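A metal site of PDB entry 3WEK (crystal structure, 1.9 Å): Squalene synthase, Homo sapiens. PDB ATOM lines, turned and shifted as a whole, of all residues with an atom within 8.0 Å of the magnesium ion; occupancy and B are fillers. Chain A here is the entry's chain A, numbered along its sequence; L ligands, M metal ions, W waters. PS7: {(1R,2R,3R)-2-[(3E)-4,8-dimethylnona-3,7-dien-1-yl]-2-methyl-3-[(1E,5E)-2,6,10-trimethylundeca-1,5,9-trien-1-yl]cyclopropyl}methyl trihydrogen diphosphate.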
ATOM      1  N   LEU A  49      16.304  22.482 -20.701  1.00  0.00           N
ATOM      2  CA  LEU A  49      14.866  22.472 -20.917  1.00  0.00           C
ATOM      3  C   LEU A  49      14.534  22.287 -22.384  1.00  0.00           C
ATOM      4  O   LEU A  49      13.539  21.628 -22.708  1.00  0.00           O
ATOM      5  CB  LEU A  49      14.236  23.740 -20.322  1.00  0.00           C
ATOM      6  CG  LEU A  49      14.271  23.825 -18.790  1.00  0.00           C
ATOM      7  CD1 LEU A  49      13.464  25.019 -18.351  1.00  0.00           C
ATOM      8  CD2 LEU A  49      13.819  22.577 -18.046  1.00  0.00           C
ATOM      9  N   ARG A  50      15.351  22.845 -23.276  1.00  0.00           N
ATOM     10  CA  ARG A  50      15.180  22.583 -24.698  1.00  0.00           C
ATOM     11  C   ARG A  50      15.338  21.089 -25.016  1.00  0.00           C
ATOM     12  O   ARG A  50      14.553  20.532 -25.775  1.00  0.00           O
ATOM     13  CB  ARG A  50      16.119  23.480 -25.520  1.00  0.00           C
ATOM     14  CG  ARG A  50      16.105  23.268 -27.030  1.00  0.00           C
ATOM     15  CD  ARG A  50      14.699  23.379 -27.587  1.00  0.00           C
ATOM     16  NE  ARG A  50      14.193  24.737 -27.587  1.00  0.00           N
ATOM     17  CZ  ARG A  50      12.893  25.044 -27.638  1.00  0.00           C
ATOM     18  NH1 ARG A  50      11.983  24.073 -27.682  1.00  0.00           N
ATOM     19  NH2 ARG A  50      12.511  26.314 -27.668  1.00  0.00           N
ATOM     20  N   LEU A  52      14.849  18.517 -22.851  1.00  0.00           N
ATOM     21  CA  LEU A  52      13.683  17.867 -22.264  1.00  0.00           C
ATOM     22  C   LEU A  52      12.455  18.011 -23.165  1.00  0.00           C
ATOM     23  O   LEU A  52      11.710  17.049 -23.383  1.00  0.00           O
ATOM     24  CB  LEU A  52      13.394  18.410 -20.864  1.00  0.00           C
ATOM     25  CG  LEU A  52      12.231  17.811 -20.081  1.00  0.00           C
ATOM     26  CD1 LEU A  52      12.402  16.317 -19.908  1.00  0.00           C
ATOM     27  CD2 LEU A  52      12.122  18.452 -18.710  1.00  0.00           C
ATOM     28  N   ASP A  53      12.274  19.208 -23.714  1.00  0.00           N
ATOM     29  CA  ASP A  53      11.130  19.490 -24.589  1.00  0.00           C
ATOM     30  C   ASP A  53      11.217  18.730 -25.904  1.00  0.00           C
ATOM     31  O   ASP A  53      10.189  18.320 -26.451  1.00  0.00           O
ATOM     32  CB  ASP A  53      11.004  20.988 -24.890  1.00  0.00           C
ATOM     33  CG  ASP A  53       9.645  21.329 -25.487  1.00  0.00           C
ATOM     34  OD1 ASP A  53       8.623  20.970 -24.860  1.00  0.00           O
ATOM     35  OD2 ASP A  53       9.597  21.924 -26.583  1.00  0.00           O
ATOM     36  N   THR A  54      12.448  18.545 -26.396  1.00  0.00           N
ATOM     37  CA  THR A  54      12.688  17.882 -27.671  1.00  0.00           C
ATOM     38  C   THR A  54      12.279  16.422 -27.584  1.00  0.00           C
ATOM     39  O   THR A  54      11.832  15.831 -28.575  1.00  0.00           O
ATOM     40  CB  THR A  54      14.156  18.032 -28.142  1.00  0.00           C
ATOM     41  OG1 THR A  54      14.493  19.423 -28.233  1.00  0.00           O
ATOM     42  CG2 THR A  54      14.348  17.396 -29.515  1.00  0.00           C
ATOM     43  N   LEU A  55      12.438  15.852 -26.393  1.00  0.00           N
ATOM     44  CA  LEU A  55      11.918  14.535 -26.045  1.00  0.00           C
ATOM     45  C   LEU A  55      10.394  14.528 -25.949  1.00  0.00           C
ATOM     46  O   LEU A  55       9.742  13.709 -26.584  1.00  0.00           O
ATOM     47  CB  LEU A  55      12.507  14.039 -24.727  1.00  0.00           C
ATOM     48  CG  LEU A  55      13.937  13.504 -24.722  1.00  0.00           C
ATOM     49  CD1 LEU A  55      14.385  13.204 -23.294  1.00  0.00           C
ATOM     50  CD2 LEU A  55      14.093  12.273 -25.604  1.00  0.00           C
ATOM     51  N   GLU A  56       9.838  15.453 -25.159  1.00  0.00           N
ATOM     52  CA  GLU A  56       8.390  15.496 -24.958  1.00  0.00           C
ATOM     53  C   GLU A  56       7.651  15.563 -26.294  1.00  0.00           C
ATOM     54  O   GLU A  56       6.617  14.917 -26.453  1.00  0.00           O
ATOM     55  CB  GLU A  56       7.973  16.666 -24.066  1.00  0.00           C
ATOM     56  CG  GLU A  56       6.515  16.597 -23.601  1.00  0.00           C
ATOM     57  CD  GLU A  56       5.766  17.925 -23.632  1.00  0.00           C
ATOM     58  OE1 GLU A  56       6.232  18.897 -24.272  1.00  0.00           O
ATOM     59  OE2 GLU A  56       4.694  18.000 -23.008  1.00  0.00           O
ATOM     60  N   ASP A  57       8.202  16.317 -27.243  1.00  0.00           N
ATOM     61  CA  ASP A  57       7.515  16.684 -28.470  1.00  0.00           C
ATOM     62  C   ASP A  57       7.636  15.693 -29.610  1.00  0.00           C
ATOM     63  O   ASP A  57       6.852  15.747 -30.556  1.00  0.00           O
ATOM     64  CB  ASP A  57       8.037  18.028 -28.980  1.00  0.00           C
ATOM     65  CG  ASP A  57       7.459  19.202 -28.219  1.00  0.00           C
ATOM     66  OD1 ASP A  57       6.884  19.033 -27.119  1.00  0.00           O
ATOM     67  OD2 ASP A  57       7.613  20.328 -28.724  1.00  0.00           O
ATOM     68  N   ASP A  58       8.647  14.834 -29.536  1.00  0.00           N
ATOM     69  CA  ASP A  58       8.941  13.840 -30.563  1.00  0.00           C
ATOM     70  C   ASP A  58       7.859  12.773 -30.503  1.00  0.00           C
ATOM     71  O   ASP A  58       7.720  12.073 -29.500  1.00  0.00           O
ATOM     72  CB  ASP A  58      10.328  13.234 -30.323  1.00  0.00           C
ATOM     73  CG  ASP A  58      10.887  12.516 -31.542  1.00  0.00           C
ATOM     74  OD1 ASP A  58      10.140  12.298 -32.515  1.00  0.00           O
ATOM     75  OD2 ASP A  58      12.084  12.164 -31.516  1.00  0.00           O
ATOM     76  N   MET A 123       9.206  19.343 -14.060  1.00  0.00           N
ATOM     77  CA  MET A 123       8.688  19.442 -15.402  1.00  0.00           C
ATOM     78  C   MET A 123       8.490  18.051 -16.025  1.00  0.00           C
ATOM     79  O   MET A 123       7.463  17.782 -16.628  1.00  0.00           O
ATOM     80  CB  MET A 123       9.594  20.314 -16.270  1.00  0.00           C
ATOM     81  CG  MET A 123       9.089  20.491 -17.672  1.00  0.00           C
ATOM     82  SD  MET A 123       9.984  21.709 -18.645  1.00  0.00           S
ATOM     83  CE  MET A 123      10.045  23.080 -17.495  1.00  0.00           C
ATOM     84  N   MET A 127       5.080  16.733 -17.595  1.00  0.00           N
ATOM     85  CA  MET A 127       4.947  16.374 -19.004  1.00  0.00           C
ATOM     86  C   MET A 127       4.488  14.915 -19.183  1.00  0.00           C
ATOM     87  O   MET A 127       3.649  14.626 -20.037  1.00  0.00           O
ATOM     88  CB  MET A 127       6.280  16.560 -19.718  1.00  0.00           C
ATOM     89  CG  MET A 127       6.643  17.995 -20.014  1.00  0.00           C
ATOM     90  SD  MET A 127       8.404  18.025 -20.380  1.00  0.00           S
ATOM     91  CE  MET A 127       8.489  19.438 -21.457  1.00  0.00           C
ATOM     92  N   TYR A 144      -1.226  22.318 -17.247  1.00  0.00           N
ATOM     93  CA  TYR A 144      -0.288  21.963 -18.310  1.00  0.00           C
ATOM     94  C   TYR A 144       0.767  23.067 -18.516  1.00  0.00           C
ATOM     95  O   TYR A 144       1.963  22.804 -18.591  1.00  0.00           O
ATOM     96  CB  TYR A 144      -0.978  21.659 -19.646  1.00  0.00           C
ATOM     97  CG  TYR A 144       0.050  21.284 -20.685  1.00  0.00           C
ATOM     98  CD1 TYR A 144       0.798  20.115 -20.545  1.00  0.00           C
ATOM     99  CD2 TYR A 144       0.301  22.095 -21.780  1.00  0.00           C
ATOM    100  CE1 TYR A 144       1.758  19.752 -21.467  1.00  0.00           C
ATOM    101  CE2 TYR A 144       1.268  21.746 -22.718  1.00  0.00           C
ATOM    102  CZ  TYR A 144       1.979  20.575 -22.555  1.00  0.00           C
ATOM    103  OH  TYR A 144       2.961  20.193 -23.457  1.00  0.00           O
ATOM    104  N   VAL A 148       5.048  23.165 -18.207  1.00  0.00           N
ATOM    105  CA  VAL A 148       5.967  23.465 -19.300  1.00  0.00           C
ATOM    106  C   VAL A 148       6.491  24.906 -19.399  1.00  0.00           C
ATOM    107  O   VAL A 148       7.386  25.197 -20.202  1.00  0.00           O
ATOM    108  CB  VAL A 148       5.422  23.001 -20.692  1.00  0.00           C
ATOM    109  CG1 VAL A 148       5.026  21.517 -20.652  1.00  0.00           C
ATOM    110  CG2 VAL A 148       4.230  23.856 -21.148  1.00  0.00           C
ATOM    111  N   GLN A 185       3.117  31.151 -22.646  1.00  0.00           N
ATOM    112  CA  GLN A 185       2.736  29.822 -23.101  1.00  0.00           C
ATOM    113  C   GLN A 185       1.313  29.840 -23.645  1.00  0.00           C
ATOM    114  O   GLN A 185       1.081  29.319 -24.728  1.00  0.00           O
ATOM    115  CB  GLN A 185       2.864  28.788 -21.964  1.00  0.00           C
ATOM    116  CG  GLN A 185       2.580  27.324 -22.414  1.00  0.00           C
ATOM    117  CD  GLN A 185       3.606  26.783 -23.395  1.00  0.00           C
ATOM    118  OE1 GLN A 185       4.638  26.256 -22.987  1.00  0.00           O
ATOM    119  NE2 GLN A 185       3.353  26.932 -24.695  1.00  0.00           N
ATOM    120  N   ARG A 201      -1.209  17.882 -32.574  1.00  0.00           N
ATOM    121  CA  ARG A 201      -1.165  18.285 -31.162  1.00  0.00           C
ATOM    122  C   ARG A 201      -2.335  19.230 -30.885  1.00  0.00           C
ATOM    123  O   ARG A 201      -2.653  20.075 -31.724  1.00  0.00           O
ATOM    124  CB  ARG A 201       0.149  18.988 -30.818  1.00  0.00           C
ATOM    125  CG  ARG A 201       1.208  18.978 -31.915  1.00  0.00           C
ATOM    126  CD  ARG A 201       2.492  19.677 -31.494  1.00  0.00           C
ATOM    127  NE  ARG A 201       2.867  20.765 -32.397  1.00  0.00           N
ATOM    128  CZ  ARG A 201       3.335  20.613 -33.634  1.00  0.00           C
ATOM    129  NH1 ARG A 201       3.501  19.401 -34.157  1.00  0.00           N
ATOM    130  NH2 ARG A 201       3.641  21.677 -34.357  1.00  0.00           N
ATOM    131  N   PHE A 203      -3.926  21.768 -27.789  1.00  0.00           N
ATOM    132  CA  PHE A 203      -3.661  22.418 -26.502  1.00  0.00           C
ATOM    133  C   PHE A 203      -4.768  23.325 -25.945  1.00  0.00           C
ATOM    134  O   PHE A 203      -4.754  23.645 -24.766  1.00  0.00           O
ATOM    135  CB  PHE A 203      -2.342  23.203 -26.580  1.00  0.00           C
ATOM    136  CG  PHE A 203      -1.142  22.336 -26.849  1.00  0.00           C
ATOM    137  CD1 PHE A 203      -0.575  21.571 -25.846  1.00  0.00           C
ATOM    138  CD2 PHE A 203      -0.543  22.340 -28.108  1.00  0.00           C
ATOM    139  CE1 PHE A 203       0.552  20.782 -26.099  1.00  0.00           C
ATOM    140  CE2 PHE A 203       0.580  21.561 -28.379  1.00  0.00           C
ATOM    141  CZ  PHE A 203       1.137  20.778 -27.374  1.00  0.00           C
HETATM  142  CAA PS7 L   1      14.718  31.470 -20.842  1.00  0.00           C
HETATM  143  CAB PS7 L   1      15.278  29.325 -19.332  1.00  0.00           C
HETATM  144  CAC PS7 L   1       9.968  34.713 -14.554  1.00  0.00           C
HETATM  145  CAD PS7 L   1      10.936  35.494 -16.913  1.00  0.00           C
HETATM  146  CAE PS7 L   1      13.052  25.603 -23.635  1.00  0.00           C
HETATM  147  CAF PS7 L   1      10.686  32.016 -20.517  1.00  0.00           C
HETATM  148  CAG PS7 L   1       9.528  24.898 -24.832  1.00  0.00           C
HETATM  149  CAH PS7 L   1       6.631  29.619 -24.049  1.00  0.00           C
HETATM  150  OAI PS7 L   1      13.024  31.227 -29.477  1.00  0.00           O
HETATM  151  OAJ PS7 L   1       9.321  32.079 -28.013  1.00  0.00           O
HETATM  152  OAK PS7 L   1      12.013  29.000 -30.158  1.00  0.00           O
HETATM  153  OAL PS7 L   1      10.612  31.122 -30.351  1.00  0.00           O
HETATM  154  OAM PS7 L   1       8.851  29.659 -28.639  1.00  0.00           O
HETATM  155  CAN PS7 L   1      13.780  29.210 -21.356  1.00  0.00           C
HETATM  156  CAO PS7 L   1       9.217  33.627 -16.691  1.00  0.00           C
HETATM  157  CAP PS7 L   1      11.138  25.379 -21.869  1.00  0.00           C
HETATM  158  CAQ PS7 L   1       8.747  30.480 -20.302  1.00  0.00           C
HETATM  159  CAR PS7 L   1       8.155  26.195 -23.117  1.00  0.00           C
HETATM  160  CAS PS7 L   1      13.480  27.862 -21.299  1.00  0.00           C
HETATM  161  CAT PS7 L   1       9.079  33.291 -18.030  1.00  0.00           C
HETATM  162  CAU PS7 L   1      10.709  24.065 -22.001  1.00  0.00           C
HETATM  163  CAV PS7 L   1       8.916  30.080 -21.634  1.00  0.00           C
HETATM  164  CAW PS7 L   1      12.254  27.595 -22.158  1.00  0.00           C
HETATM  165  CAX PS7 L   1       9.374  31.793 -18.213  1.00  0.00           C
HETATM  166  CAY PS7 L   1       9.223  23.984 -22.396  1.00  0.00           C
HETATM  167  CAZ PS7 L   1       8.800  28.917 -25.885  1.00  0.00           C
HETATM  168  CBA PS7 L   1       8.074  28.857 -22.001  1.00  0.00           C
HETATM  169  OBB PS7 L   1       9.307  30.245 -26.126  1.00  0.00           O
HETATM  170  OBC PS7 L   1      11.185  30.265 -27.991  1.00  0.00           O
HETATM  171  CBD PS7 L   1      14.593  29.971 -20.543  1.00  0.00           C
HETATM  172  CBE PS7 L   1      10.026  34.589 -16.077  1.00  0.00           C
HETATM  173  CBF PS7 L   1      12.112  26.127 -22.545  1.00  0.00           C
HETATM  174  CBG PS7 L   1       9.572  31.408 -19.683  1.00  0.00           C
HETATM  175  CBH PS7 L   1       8.910  25.066 -23.443  1.00  0.00           C
HETATM  176  CBI PS7 L   1       7.825  27.335 -24.108  1.00  0.00           C
HETATM  177  CBJ PS7 L   1       8.903  28.382 -24.442  1.00  0.00           C
HETATM  178  CBK PS7 L   1       7.752  28.728 -23.502  1.00  0.00           C
HETATM  179  PBL PS7 L   1      11.728  30.299 -29.520  1.00  0.00           P
HETATM  180  PBM PS7 L   1       9.654  30.673 -27.671  1.00  0.00           P
HETATM  181 MG    MG M   1       6.478  20.563 -25.708  1.00  0.00          MG
HETATM  182  O   HOH W   1       6.251  21.911 -24.521  1.00  0.00           O
HETATM  183  O   HOH W   2       6.857  22.222 -27.148  1.00  0.00           O
HETATM  184  O   HOH W   3       4.233  20.554 -25.932  1.00  0.00           O
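Water W2 bridges OD2 of Asp 57 (2.6 Å) and OD2 of Asp 53 (2.8 Å).
The magnesium ion is bound by water W1 (1.8 Å), OD1 of Asp 57 (2.1 Å), OE1 of Glu 56 (2.2 Å), water W2 (2.2 Å), water W3 (2.3 Å) and OD1 of Asp 53 (2.3 Å). The magnesium ion has six donor atoms within binding distance.
The side-chain carboxylate (OE2) of Glu 56 lies within hydrogen-bond range of the side-chain hydroxyl (OH) of Tyr 144 (2.8 Å). OD2 of Asp 53 is in salt-bridge range of NH1 of Arg 50 (3.4 Å).
NH2 of Arg 50 is in salt-bridge range of OAK of the ligand, at 3.7 Å.
Within 4 Å of the magnesium ion: Asp 53, Glu 56 and Asp 57.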
